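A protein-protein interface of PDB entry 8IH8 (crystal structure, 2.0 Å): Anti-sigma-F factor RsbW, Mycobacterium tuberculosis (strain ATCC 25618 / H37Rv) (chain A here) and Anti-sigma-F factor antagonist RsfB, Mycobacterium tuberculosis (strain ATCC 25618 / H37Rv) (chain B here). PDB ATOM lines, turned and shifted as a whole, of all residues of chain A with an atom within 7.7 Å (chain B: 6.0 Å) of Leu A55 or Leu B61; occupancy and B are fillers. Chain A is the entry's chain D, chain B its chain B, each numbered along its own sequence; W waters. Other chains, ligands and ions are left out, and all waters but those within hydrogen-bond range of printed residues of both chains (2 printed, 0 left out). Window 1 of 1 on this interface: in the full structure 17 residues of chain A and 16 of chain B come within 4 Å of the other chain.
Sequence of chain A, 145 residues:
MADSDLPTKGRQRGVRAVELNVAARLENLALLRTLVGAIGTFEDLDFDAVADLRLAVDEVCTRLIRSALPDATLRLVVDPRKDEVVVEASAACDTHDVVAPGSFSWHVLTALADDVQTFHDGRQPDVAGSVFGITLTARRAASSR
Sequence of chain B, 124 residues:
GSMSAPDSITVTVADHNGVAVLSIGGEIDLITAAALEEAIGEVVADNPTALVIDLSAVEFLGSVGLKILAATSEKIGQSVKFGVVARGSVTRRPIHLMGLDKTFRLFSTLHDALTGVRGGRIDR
The guanidinium group (NH2) of Arg A33 lies within salt-bridge range of the side-chain carboxylate (OE1) of Glu B27 (2.7 Å). The side-chain carboxylate of Glu B27 lies within salt-bridge range of the guanidinium group of Arg A54 (3.0 Å). The guanidinium group (NH2) of Arg A54 is in hydrogen-bond range of the backbone carbonyl oxygen (O) of Glu B59, 3.2 Å away. The side-chain hydroxyl of Ser B63 sits at hydrogen-bond distance from the side-chain carboxylate of Glu A59 (2.6 Å).
The backbone NH (N) of Glu B59 sits at hydrogen-bond distance from the backbone carbonyl oxygen (O) of Gly B26, 2.7 Å away. N of Ile B28 is in hydrogen-bond range of O of Phe B60 (2.8 Å). N of Gly B62 is in hydrogen-bond range of O of Ile B28 (2.8 Å). O of Arg A33 lies within hydrogen-bond range of NH1 of Arg A54, 3.2 Å away. NH1 of Arg A33 lies within salt-bridge range of OD1 of Asp A58, at 2.9 Å. The backbone carbonyl oxygen of Asp A58 is in hydrogen-bond range of the side-chain hydroxyl of Thr A62 (2.8 Å).
Arg A33 touches Phe B60 (CD to CE2, 3.6 Å). Phe B60 touches Arg A54. Leu A55 touches Phe B60 (CD1 to CZ, 3.8 Å). Leu A55 touches Leu B61 (CD1 to O, 3.6 Å). Gly B62 touches Leu A55. Leu A55 touches Ser B63. Leu A55 touches Pro B94. OD2 of Asp A58 touches CZ of Phe B60 (3.4 Å). CG2 of Val A108 touches CB of Ser B63, at 3.996 Å.
Of the printed residues of chain B, Arg A33 touches Glu B27 (2.7 Å) and Phe B60 (3.6 Å). Of the printed residues of chain B, Arg A54 touches Glu B27 (3.0 Å), Glu B59 (3.2 Å) and Phe B60 (3.5 Å). Leu A55 touches just these residues of chain B: Phe B60 (3.8 Å), Leu B61 (3.6 Å), Gly B62 (3.8 Å), Ser B63 (3.9 Å) and Pro B94 (3.6 Å). Printed residues of chain B within 4 Å of Glu A59: Ser B63. Leu A112 touches none of the printed residues of chain B. Of the printed residues of chain A, Glu B27 touches Arg A33 and Arg A54. Of the printed residues of chain A, Glu B59 touches Arg A54. Of chain A, only Leu A55 (3.6 Å) comes within 4 Å of Leu B61. Gly B62 touches one residue of chain A. The nearest residue of chain B that does not touch Leu A55 is Leu B66 (4.7 Å). The nearest residue of chain A that does not touch Leu B61 is Arg A54 (6.2 Å). The nearest printed residue of chain B that does not touch Arg A33 is Ile B28 (5.8 Å).
Printed residues of chain A that touch a printed residue of chain B: Arg A33, Arg A54, Leu A55, Asp A58, Glu A59 and Val A108. Among the printed residues, 13 pairs touch across the chains.
Water W1 lies within hydrogen-bond range of the side-chain carboxylate of Asp A58 (2.7 Å), the side-chain carboxylate of Glu A59 (2.8 Å) and the backbone NH of Ser B63 (3.0 Å). Water W2 lies within hydrogen-bond range of the guanidinium group (NH1) of Arg A54 (2.7 Å) and the side-chain carboxylate (OE2) of Glu B27 (3.0 Å).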
ATOM      1  N   ARG A  33     -28.304   8.892 -13.874  1.00  0.00           N
ATOM      2  CA  ARG A  33     -26.910   9.315 -13.761  1.00  0.00           C
ATOM      3  C   ARG A  33     -26.474  10.114 -14.969  1.00  0.00           C
ATOM      4  O   ARG A  33     -25.684  11.060 -14.851  1.00  0.00           O
ATOM      5  CB  ARG A  33     -25.978   8.113 -13.638  1.00  0.00           C
ATOM      6  CG  ARG A  33     -25.946   7.497 -12.326  1.00  0.00           C
ATOM      7  CD  ARG A  33     -24.694   6.672 -12.205  1.00  0.00           C
ATOM      8  NE  ARG A  33     -24.585   5.615 -13.212  1.00  0.00           N
ATOM      9  CZ  ARG A  33     -25.168   4.423 -13.100  1.00  0.00           C
ATOM     10  NH1 ARG A  33     -25.952   4.157 -12.048  1.00  0.00           N
ATOM     11  NH2 ARG A  33     -24.972   3.497 -14.038  1.00  0.00           N
ATOM     12  N   VAL A  36     -28.048  13.574 -14.708  1.00  0.00           N
ATOM     13  CA  VAL A  36     -27.386  14.367 -13.662  1.00  0.00           C
ATOM     14  C   VAL A  36     -26.025  14.862 -14.147  1.00  0.00           C
ATOM     15  O   VAL A  36     -25.632  16.010 -13.884  1.00  0.00           O
ATOM     16  CB  VAL A  36     -27.247  13.547 -12.361  1.00  0.00           C
ATOM     17  CG1 VAL A  36     -26.316  14.248 -11.361  1.00  0.00           C
ATOM     18  CG2 VAL A  36     -28.603  13.328 -11.710  1.00  0.00           C
ATOM     19  N   ALA A  49     -16.359  18.096  -9.365  1.00  0.00           N
ATOM     20  CA  ALA A  49     -17.705  18.413  -8.899  1.00  0.00           C
ATOM     21  C   ALA A  49     -18.763  17.639  -9.676  1.00  0.00           C
ATOM     22  O   ALA A  49     -19.770  17.203  -9.098  1.00  0.00           O
ATOM     23  CB  ALA A  49     -17.955  19.917  -9.004  1.00  0.00           C
ATOM     24  N   VAL A  50     -18.560  17.448 -10.985  1.00  0.00           N
ATOM     25  CA  VAL A  50     -19.526  16.651 -11.751  1.00  0.00           C
ATOM     26  C   VAL A  50     -19.538  15.205 -11.258  1.00  0.00           C
ATOM     27  O   VAL A  50     -20.601  14.594 -11.089  1.00  0.00           O
ATOM     28  CB  VAL A  50     -19.229  16.736 -13.261  1.00  0.00           C
ATOM     29  CG1 VAL A  50     -20.085  15.740 -14.026  1.00  0.00           C
ATOM     30  CG2 VAL A  50     -19.508  18.140 -13.752  1.00  0.00           C
ATOM     31  N   ALA A  51     -18.361  14.640 -11.007  1.00  0.00           N
ATOM     32  CA  ALA A  51     -18.307  13.272 -10.512  1.00  0.00           C
ATOM     33  C   ALA A  51     -18.891  13.178  -9.104  1.00  0.00           C
ATOM     34  O   ALA A  51     -19.600  12.214  -8.790  1.00  0.00           O
ATOM     35  CB  ALA A  51     -16.864  12.759 -10.555  1.00  0.00           C
ATOM     36  N   ASP A  52     -18.610  14.174  -8.247  1.00  0.00           N
ATOM     37  CA  ASP A  52     -19.177  14.196  -6.901  1.00  0.00           C
ATOM     38  C   ASP A  52     -20.700  14.208  -6.963  1.00  0.00           C
ATOM     39  O   ASP A  52     -21.376  13.486  -6.219  1.00  0.00           O
ATOM     40  CB  ASP A  52     -18.693  15.426  -6.114  1.00  0.00           C
ATOM     41  CG  ASP A  52     -17.201  15.371  -5.695  1.00  0.00           C
ATOM     42  OD1 ASP A  52     -16.478  14.372  -5.937  1.00  0.00           O
ATOM     43  OD2 ASP A  52     -16.748  16.381  -5.104  1.00  0.00           O
ATOM     44  N   LEU A  53     -21.251  15.031  -7.847  1.00  0.00           N
ATOM     45  CA  LEU A  53     -22.695  15.146  -8.010  1.00  0.00           C
ATOM     46  C   LEU A  53     -23.306  13.848  -8.527  1.00  0.00           C
ATOM     47  O   LEU A  53     -24.338  13.385  -8.027  1.00  0.00           O
ATOM     48  CB  LEU A  53     -22.994  16.291  -8.985  1.00  0.00           C
ATOM     49  CG  LEU A  53     -24.468  16.650  -9.152  1.00  0.00           C
ATOM     50  CD1 LEU A  53     -25.007  17.219  -7.836  1.00  0.00           C
ATOM     51  CD2 LEU A  53     -24.704  17.611 -10.353  1.00  0.00           C
ATOM     52  N   ARG A  54     -22.703  13.268  -9.562  1.00  0.00           N
ATOM     53  CA  ARG A  54     -23.199  12.001 -10.088  1.00  0.00           C
ATOM     54  C   ARG A  54     -23.243  10.927  -9.007  1.00  0.00           C
ATOM     55  O   ARG A  54     -24.219  10.178  -8.907  1.00  0.00           O
ATOM     56  CB  ARG A  54     -22.325  11.535 -11.245  1.00  0.00           C
ATOM     57  CG  ARG A  54     -22.886  11.853 -12.603  1.00  0.00           C
ATOM     58  CD  ARG A  54     -21.800  11.860 -13.632  1.00  0.00           C
ATOM     59  NE  ARG A  54     -21.184  10.555 -13.849  1.00  0.00           N
ATOM     60  CZ  ARG A  54     -21.663   9.620 -14.665  1.00  0.00           C
ATOM     61  NH1 ARG A  54     -22.792   9.821 -15.325  1.00  0.00           N
ATOM     62  NH2 ARG A  54     -21.004   8.474 -14.825  1.00  0.00           N
ATOM     63  N   LEU A  55     -22.169  10.802  -8.222  1.00  0.00           N
ATOM     64  CA  LEU A  55     -22.109   9.745  -7.220  1.00  0.00           C
ATOM     65  C   LEU A  55     -23.119   9.995  -6.108  1.00  0.00           C
ATOM     66  O   LEU A  55     -23.829   9.078  -5.672  1.00  0.00           O
ATOM     67  CB  LEU A  55     -20.693   9.661  -6.642  1.00  0.00           C
ATOM     68  CG  LEU A  55     -20.409   8.572  -5.617  1.00  0.00           C
ATOM     69  CD1 LEU A  55     -21.025   7.256  -6.030  1.00  0.00           C
ATOM     70  CD2 LEU A  55     -18.902   8.396  -5.395  1.00  0.00           C
ATOM     71  N   ALA A  56     -23.162  11.227  -5.606  1.00  0.00           N
ATOM     72  CA  ALA A  56     -24.095  11.545  -4.529  1.00  0.00           C
ATOM     73  C   ALA A  56     -25.539  11.342  -4.977  1.00  0.00           C
ATOM     74  O   ALA A  56     -26.348  10.771  -4.240  1.00  0.00           O
ATOM     75  CB  ALA A  56     -23.870  12.983  -4.050  1.00  0.00           C
ATOM     76  N   VAL A  57     -25.886  11.788  -6.189  1.00  0.00           N
ATOM     77  CA  VAL A  57     -27.280  11.627  -6.602  1.00  0.00           C
ATOM     78  C   VAL A  57     -27.573  10.173  -6.965  1.00  0.00           C
ATOM     79  O   VAL A  57     -28.707   9.705  -6.782  1.00  0.00           O
ATOM     80  CB  VAL A  57     -27.655  12.578  -7.760  1.00  0.00           C
ATOM     81  CG1 VAL A  57     -29.134  12.389  -8.166  1.00  0.00           C
ATOM     82  CG2 VAL A  57     -27.471  14.033  -7.347  1.00  0.00           C
ATOM     83  N   ASP A  58     -26.597   9.454  -7.527  1.00  0.00           N
ATOM     84  CA  ASP A  58     -26.779   8.024  -7.745  1.00  0.00           C
ATOM     85  C   ASP A  58     -27.050   7.308  -6.427  1.00  0.00           C
ATOM     86  O   ASP A  58     -27.872   6.385  -6.372  1.00  0.00           O
ATOM     87  CB  ASP A  58     -25.546   7.404  -8.405  1.00  0.00           C
ATOM     88  CG  ASP A  58     -25.689   5.893  -8.591  1.00  0.00           C
ATOM     89  OD1 ASP A  58     -26.423   5.454  -9.502  1.00  0.00           O
ATOM     90  OD2 ASP A  58     -25.085   5.129  -7.819  1.00  0.00           O
ATOM     91  N   GLU A  59     -26.341   7.699  -5.361  1.00  0.00           N
ATOM     92  CA  GLU A  59     -26.577   7.076  -4.062  1.00  0.00           C
ATOM     93  C   GLU A  59     -28.011   7.303  -3.593  1.00  0.00           C
ATOM     94  O   GLU A  59     -28.681   6.365  -3.144  1.00  0.00           O
ATOM     95  CB  GLU A  59     -25.581   7.588  -3.018  1.00  0.00           C
ATOM     96  CG  GLU A  59     -25.693   6.884  -1.667  1.00  0.00           C
ATOM     97  CD  GLU A  59     -25.357   5.398  -1.773  1.00  0.00           C
ATOM     98  OE1 GLU A  59     -25.734   4.614  -0.863  1.00  0.00           O
ATOM     99  OE2 GLU A  59     -24.755   5.014  -2.805  1.00  0.00           O
ATOM    100  N   VAL A  60     -28.505   8.542  -3.674  1.00  0.00           N
ATOM    101  CA  VAL A  60     -29.857   8.780  -3.170  1.00  0.00           C
ATOM    102  C   VAL A  60     -30.889   8.097  -4.053  1.00  0.00           C
ATOM    103  O   VAL A  60     -31.888   7.571  -3.553  1.00  0.00           O
ATOM    104  CB  VAL A  60     -30.158  10.287  -3.002  1.00  0.00           C
ATOM    105  CG1 VAL A  60     -29.056  10.990  -2.169  1.00  0.00           C
ATOM    106  CG2 VAL A  60     -30.346  10.946  -4.322  1.00  0.00           C
ATOM    107  N   CYS A  61     -30.663   8.073  -5.376  1.00  0.00           N
ATOM    108  CA  CYS A  61     -31.621   7.430  -6.265  1.00  0.00           C
ATOM    109  C   CYS A  61     -31.631   5.917  -6.074  1.00  0.00           C
ATOM    110  O   CYS A  61     -32.694   5.283  -6.119  1.00  0.00           O
ATOM    111  CB  CYS A  61     -31.296   7.786  -7.718  1.00  0.00           C
ATOM    112  SG  CYS A  61     -31.667   9.512  -8.107  1.00  0.00           S
ATOM    113  N   THR A  62     -30.458   5.314  -5.867  1.00  0.00           N
ATOM    114  CA  THR A  62     -30.409   3.888  -5.567  1.00  0.00           C
ATOM    115  C   THR A  62     -31.215   3.568  -4.315  1.00  0.00           C
ATOM    116  O   THR A  62     -32.007   2.621  -4.303  1.00  0.00           O
ATOM    117  CB  THR A  62     -28.958   3.420  -5.405  1.00  0.00           C
ATOM    118  OG1 THR A  62     -28.261   3.635  -6.636  1.00  0.00           O
ATOM    119  CG2 THR A  62     -28.882   1.912  -4.996  1.00  0.00           C
ATOM    120  N   VAL A 108     -21.041   8.205   2.472  1.00  0.00           N
ATOM    121  CA  VAL A 108     -20.835   8.645   1.094  1.00  0.00           C
ATOM    122  C   VAL A 108     -21.448  10.023   0.879  1.00  0.00           C
ATOM    123  O   VAL A 108     -20.810  10.926   0.323  1.00  0.00           O
ATOM    124  CB  VAL A 108     -21.411   7.611   0.114  1.00  0.00           C
ATOM    125  CG1 VAL A 108     -21.425   8.173  -1.300  1.00  0.00           C
ATOM    126  CG2 VAL A 108     -20.580   6.321   0.163  1.00  0.00           C
ATOM    127  N   LEU A 109     -22.684  10.211   1.347  1.00  0.00           N
ATOM    128  CA  LEU A 109     -23.408  11.440   1.032  1.00  0.00           C
ATOM    129  C   LEU A 109     -22.735  12.656   1.659  1.00  0.00           C
ATOM    130  O   LEU A 109     -22.566  13.686   0.994  1.00  0.00           O
ATOM    131  CB  LEU A 109     -24.860  11.319   1.495  1.00  0.00           C
ATOM    132  CG  LEU A 109     -25.683  10.322   0.676  1.00  0.00           C
ATOM    133  CD1 LEU A 109     -27.031  10.084   1.297  1.00  0.00           C
ATOM    134  CD2 LEU A 109     -25.849  10.833  -0.766  1.00  0.00           C
ATOM    135  N   LEU A 112     -19.529  13.701  -0.137  1.00  0.00           N
ATOM    136  CA  LEU A 112     -19.633  14.239  -1.485  1.00  0.00           C
ATOM    137  C   LEU A 112     -20.521  15.462  -1.616  1.00  0.00           C
ATOM    138  O   LEU A 112     -20.452  16.139  -2.651  1.00  0.00           O
ATOM    139  CB  LEU A 112     -20.172  13.184  -2.444  1.00  0.00           C
ATOM    140  CG  LEU A 112     -19.222  12.029  -2.697  1.00  0.00           C
ATOM    141  CD1 LEU A 112     -20.081  10.858  -3.106  1.00  0.00           C
ATOM    142  CD2 LEU A 112     -18.194  12.393  -3.756  1.00  0.00           C
ATOM    143  N   LEU A 136     -29.665  17.756  -1.115  1.00  0.00           N
ATOM    144  CA  LEU A 136     -28.227  17.927  -1.012  1.00  0.00           C
ATOM    145  C   LEU A 136     -27.802  19.123  -1.847  1.00  0.00           C
ATOM    146  O   LEU A 136     -28.510  19.570  -2.761  1.00  0.00           O
ATOM    147  CB  LEU A 136     -27.483  16.650  -1.431  1.00  0.00           C
ATOM    148  CG  LEU A 136     -27.664  16.115  -2.850  1.00  0.00           C
ATOM    149  CD1 LEU A 136     -26.768  16.804  -3.866  1.00  0.00           C
ATOM    150  CD2 LEU A 136     -27.366  14.623  -2.836  1.00  0.00           C
ATOM    151  N   GLY B  26     -16.645   0.528 -18.219  1.00  0.00           N
ATOM    152  CA  GLY B  26     -18.054   0.867 -18.078  1.00  0.00           C
ATOM    153  C   GLY B  26     -18.441   1.378 -16.698  1.00  0.00           C
ATOM    154  O   GLY B  26     -17.597   1.932 -15.981  1.00  0.00           O
ATOM    155  N   GLU B  27     -19.703   1.186 -16.305  1.00  0.00           N
ATOM    156  CA  GLU B  27     -20.244   1.769 -15.081  1.00  0.00           C
ATOM    157  C   GLU B  27     -20.501   0.683 -14.041  1.00  0.00           C
ATOM    158  O   GLU B  27     -21.174  -0.317 -14.324  1.00  0.00           O
ATOM    159  CB  GLU B  27     -21.510   2.578 -15.394  1.00  0.00           C
ATOM    160  CG  GLU B  27     -21.181   3.774 -16.294  1.00  0.00           C
ATOM    161  CD  GLU B  27     -22.176   4.935 -16.198  1.00  0.00           C
ATOM    162  OE1 GLU B  27     -23.344   4.715 -15.838  1.00  0.00           O
ATOM    163  OE2 GLU B  27     -21.797   6.077 -16.522  1.00  0.00           O
ATOM    164  N   ILE B  28     -19.923   0.864 -12.848  1.00  0.00           N
ATOM    165  CA  ILE B  28     -20.104  -0.054 -11.731  1.00  0.00           C
ATOM    166  C   ILE B  28     -21.195   0.529 -10.844  1.00  0.00           C
ATOM    167  O   ILE B  28     -21.004   1.570 -10.209  1.00  0.00           O
ATOM    168  CB  ILE B  28     -18.795  -0.257 -10.956  1.00  0.00           C
ATOM    169  CG1 ILE B  28     -17.748  -0.916 -11.872  1.00  0.00           C
ATOM    170  CG2 ILE B  28     -19.035  -1.070  -9.676  1.00  0.00           C
ATOM    171  CD1 ILE B  28     -16.330  -0.877 -11.320  1.00  0.00           C
ATOM    172  N   LEU B  36     -19.139  -7.598 -11.126  1.00  0.00           N
ATOM    173  CA  LEU B  36     -17.817  -7.259 -10.626  1.00  0.00           C
ATOM    174  C   LEU B  36     -17.398  -8.225  -9.531  1.00  0.00           C
ATOM    175  O   LEU B  36     -16.251  -8.688  -9.492  1.00  0.00           O
ATOM    176  CB  LEU B  36     -17.807  -5.834 -10.088  1.00  0.00           C
ATOM    177  CG  LEU B  36     -16.499  -5.353  -9.461  1.00  0.00           C
ATOM    178  CD1 LEU B  36     -15.386  -5.335 -10.474  1.00  0.00           C
ATOM    179  CD2 LEU B  36     -16.689  -3.974  -8.836  1.00  0.00           C
ATOM    180  N   LEU B  55      -9.018   0.059 -12.814  1.00  0.00           N
ATOM    181  CA  LEU B  55     -10.237   0.837 -13.027  1.00  0.00           C
ATOM    182  C   LEU B  55     -10.021   1.986 -14.007  1.00  0.00           C
ATOM    183  O   LEU B  55     -10.790   2.953 -14.000  1.00  0.00           O
ATOM    184  CB  LEU B  55     -10.758   1.366 -11.692  1.00  0.00           C
ATOM    185  CG  LEU B  55     -10.926   0.323 -10.568  1.00  0.00           C
ATOM    186  CD1 LEU B  55     -11.496   0.986  -9.323  1.00  0.00           C
ATOM    187  CD2 LEU B  55     -11.819  -0.813 -11.015  1.00  0.00           C
ATOM    188  N   VAL B  58     -13.108   2.707 -16.168  1.00  0.00           N
ATOM    189  CA  VAL B  58     -14.367   2.741 -15.438  1.00  0.00           C
ATOM    190  C   VAL B  58     -14.948   4.143 -15.556  1.00  0.00           C
ATOM    191  O   VAL B  58     -14.285   5.136 -15.237  1.00  0.00           O
ATOM    192  CB  VAL B  58     -14.162   2.332 -13.974  1.00  0.00           C
ATOM    193  CG1 VAL B  58     -15.366   2.743 -13.098  1.00  0.00           C
ATOM    194  CG2 VAL B  58     -13.909   0.809 -13.872  1.00  0.00           C
ATOM    195  N   GLU B  59     -16.191   4.213 -16.008  1.00  0.00           N
ATOM    196  CA  GLU B  59     -16.892   5.437 -16.356  1.00  0.00           C
ATOM    197  C   GLU B  59     -17.705   5.963 -15.185  1.00  0.00           C
ATOM    198  O   GLU B  59     -18.060   7.141 -15.158  1.00  0.00           O
ATOM    199  CB  GLU B  59     -17.834   5.084 -17.506  1.00  0.00           C
ATOM    200  CG  GLU B  59     -17.148   5.072 -18.819  1.00  0.00           C
ATOM    201  CD  GLU B  59     -18.007   4.385 -19.887  1.00  0.00           C
ATOM    202  OE1 GLU B  59     -19.249   4.311 -19.732  1.00  0.00           O
ATOM    203  OE2 GLU B  59     -17.412   3.818 -20.831  1.00  0.00           O
ATOM    204  N   PHE B  60     -18.057   5.083 -14.256  1.00  0.00           N
ATOM    205  CA  PHE B  60     -18.757   5.439 -13.033  1.00  0.00           C
ATOM    206  C   PHE B  60     -18.449   4.376 -12.001  1.00  0.00           C
ATOM    207  O   PHE B  60     -18.532   3.183 -12.310  1.00  0.00           O
ATOM    208  CB  PHE B  60     -20.270   5.503 -13.191  1.00  0.00           C
ATOM    209  CG  PHE B  60     -20.995   5.796 -11.882  1.00  0.00           C
ATOM    210  CD1 PHE B  60     -20.991   7.074 -11.342  1.00  0.00           C
ATOM    211  CD2 PHE B  60     -21.670   4.787 -11.199  1.00  0.00           C
ATOM    212  CE1 PHE B  60     -21.659   7.354 -10.158  1.00  0.00           C
ATOM    213  CE2 PHE B  60     -22.345   5.049 -10.000  1.00  0.00           C
ATOM    214  CZ  PHE B  60     -22.337   6.333  -9.475  1.00  0.00           C
ATOM    215  N   LEU B  61     -18.156   4.808 -10.777  1.00  0.00           N
ATOM    216  CA  LEU B  61     -17.863   3.900  -9.658  1.00  0.00           C
ATOM    217  C   LEU B  61     -18.830   4.204  -8.522  1.00  0.00           C
ATOM    218  O   LEU B  61     -18.646   5.173  -7.780  1.00  0.00           O
ATOM    219  CB  LEU B  61     -16.414   4.056  -9.215  1.00  0.00           C
ATOM    220  CG  LEU B  61     -15.978   3.196  -8.021  1.00  0.00           C
ATOM    221  CD1 LEU B  61     -16.191   1.733  -8.327  1.00  0.00           C
ATOM    222  CD2 LEU B  61     -14.502   3.503  -7.671  1.00  0.00           C
ATOM    223  N   GLY B  62     -19.898   3.427  -8.406  1.00  0.00           N
ATOM    224  CA  GLY B  62     -20.874   3.689  -7.366  1.00  0.00           C
ATOM    225  C   GLY B  62     -20.382   3.245  -5.990  1.00  0.00           C
ATOM    226  O   GLY B  62     -19.318   2.644  -5.829  1.00  0.00           O
ATOM    227  N   SER B  63     -21.193   3.548  -4.974  1.00  0.00           N
ATOM    228  CA  SER B  63     -20.796   3.199  -3.613  1.00  0.00           C
ATOM    229  C   SER B  63     -20.632   1.692  -3.475  1.00  0.00           C
ATOM    230  O   SER B  63     -19.730   1.219  -2.765  1.00  0.00           O
ATOM    231  CB  SER B  63     -21.820   3.721  -2.606  1.00  0.00           C
ATOM    232  OG  SER B  63     -23.050   3.046  -2.753  1.00  0.00           O
ATOM    233  N   GLY B  65     -19.448  -0.329  -5.570  1.00  0.00           N
ATOM    234  CA  GLY B  65     -18.117  -0.687  -6.037  1.00  0.00           C
ATOM    235  C   GLY B  65     -17.051  -0.381  -5.006  1.00  0.00           C
ATOM    236  O   GLY B  65     -16.082  -1.139  -4.847  1.00  0.00           O
ATOM    237  N   LEU B  66     -17.212   0.734  -4.291  1.00  0.00           N
ATOM    238  CA  LEU B  66     -16.329   1.035  -3.167  1.00  0.00           C
ATOM    239  C   LEU B  66     -16.378  -0.076  -2.121  1.00  0.00           C
ATOM    240  O   LEU B  66     -15.336  -0.538  -1.639  1.00  0.00           O
ATOM    241  CB  LEU B  66     -16.716   2.380  -2.548  1.00  0.00           C
ATOM    242  CG  LEU B  66     -16.593   3.585  -3.492  1.00  0.00           C
ATOM    243  CD1 LEU B  66     -17.087   4.854  -2.808  1.00  0.00           C
ATOM    244  CD2 LEU B  66     -15.158   3.765  -3.965  1.00  0.00           C
ATOM    245  N   LEU B  69     -14.503  -3.198  -3.350  1.00  0.00           N
ATOM    246  CA  LEU B  69     -13.049  -3.054  -3.299  1.00  0.00           C
ATOM    247  C   LEU B  69     -12.523  -3.236  -1.878  1.00  0.00           C
ATOM    248  O   LEU B  69     -11.543  -3.957  -1.654  1.00  0.00           O
ATOM    249  CB  LEU B  69     -12.633  -1.692  -3.853  1.00  0.00           C
ATOM    250  CG  LEU B  69     -12.874  -1.492  -5.351  1.00  0.00           C
ATOM    251  CD1 LEU B  69     -12.664  -0.007  -5.716  1.00  0.00           C
ATOM    252  CD2 LEU B  69     -11.986  -2.403  -6.206  1.00  0.00           C
ATOM    253  N   VAL B  90     -13.561  10.206 -11.212  1.00  0.00           N
ATOM    254  CA  VAL B  90     -14.609   9.198 -11.126  1.00  0.00           C
ATOM    255  C   VAL B  90     -14.208   8.088 -10.183  1.00  0.00           C
ATOM    256  O   VAL B  90     -15.038   7.574  -9.426  1.00  0.00           O
ATOM    257  CB  VAL B  90     -14.902   8.645 -12.534  1.00  0.00           C
ATOM    258  CG1 VAL B  90     -15.860   7.444 -12.446  1.00  0.00           C
ATOM    259  CG2 VAL B  90     -15.445   9.742 -13.423  1.00  0.00           C
ATOM    260  N   THR B  91     -12.936   7.709 -10.241  1.00  0.00           N
ATOM    261  CA  THR B  91     -12.436   6.558  -9.511  1.00  0.00           C
ATOM    262  C   THR B  91     -11.542   6.954  -8.344  1.00  0.00           C
ATOM    263  O   THR B  91     -11.913   6.591  -7.230  1.00  0.00           O
ATOM    264  CB  THR B  91     -11.715   5.579 -10.448  1.00  0.00           C
ATOM    265  OG1 THR B  91     -10.711   6.288 -11.186  1.00  0.00           O
ATOM    266  CG2 THR B  91     -12.730   4.929 -11.400  1.00  0.00           C
ATOM    267  N   ARG B  92     -10.407   7.696  -8.498  1.00  0.00           N
ATOM    268  CA  ARG B  92      -9.547   7.536  -7.325  1.00  0.00           C
ATOM    269  C   ARG B  92     -10.180   8.498  -6.324  1.00  0.00           C
ATOM    270  O   ARG B  92     -10.023   8.363  -5.117  1.00  0.00           O
ATOM    271  CB  ARG B  92      -8.111   8.112  -7.229  1.00  0.00           C
ATOM    272  CG  ARG B  92      -7.951   9.642  -7.080  1.00  0.00           C
ATOM    273  CD  ARG B  92      -6.539  10.285  -7.082  1.00  0.00           C
ATOM    274  NE  ARG B  92      -6.005  10.183  -8.424  1.00  0.00           N
ATOM    275  CZ  ARG B  92      -4.777  10.482  -8.828  1.00  0.00           C
ATOM    276  NH1 ARG B  92      -3.803  10.721  -7.952  1.00  0.00           N
ATOM    277  NH2 ARG B  92      -4.530  10.453 -10.139  1.00  0.00           N
ATOM    278  N   PRO B  94     -13.318   9.399  -5.289  1.00  0.00           N
ATOM    279  CA  PRO B  94     -14.226   8.875  -4.252  1.00  0.00           C
ATOM    280  C   PRO B  94     -13.537   7.881  -3.338  1.00  0.00           C
ATOM    281  O   PRO B  94     -13.839   7.828  -2.135  1.00  0.00           O
ATOM    282  CB  PRO B  94     -15.348   8.198  -5.056  1.00  0.00           C
ATOM    283  CG  PRO B  94     -15.177   8.654  -6.470  1.00  0.00           C
ATOM    284  CD  PRO B  94     -13.741   9.022  -6.651  1.00  0.00           C
ATOM    285  N   ILE B  95     -12.620   7.080  -3.890  1.00  0.00           N
ATOM    286  CA  ILE B  95     -11.805   6.196  -3.055  1.00  0.00           C
ATOM    287  C   ILE B  95     -11.043   7.023  -2.033  1.00  0.00           C
ATOM    288  O   ILE B  95     -11.034   6.713  -0.835  1.00  0.00           O
ATOM    289  CB  ILE B  95     -10.848   5.363  -3.927  1.00  0.00           C
ATOM    290  CG1 ILE B  95     -11.613   4.312  -4.733  1.00  0.00           C
ATOM    291  CG2 ILE B  95      -9.766   4.689  -3.077  1.00  0.00           C
ATOM    292  CD1 ILE B  95     -10.751   3.694  -5.835  1.00  0.00           C
HETATM  293  O   HOH W   1     -23.927   4.746  -5.454  1.00  0.00           O
HETATM  294  O   HOH W   2     -23.613   8.249 -17.351  1.00  0.00           O
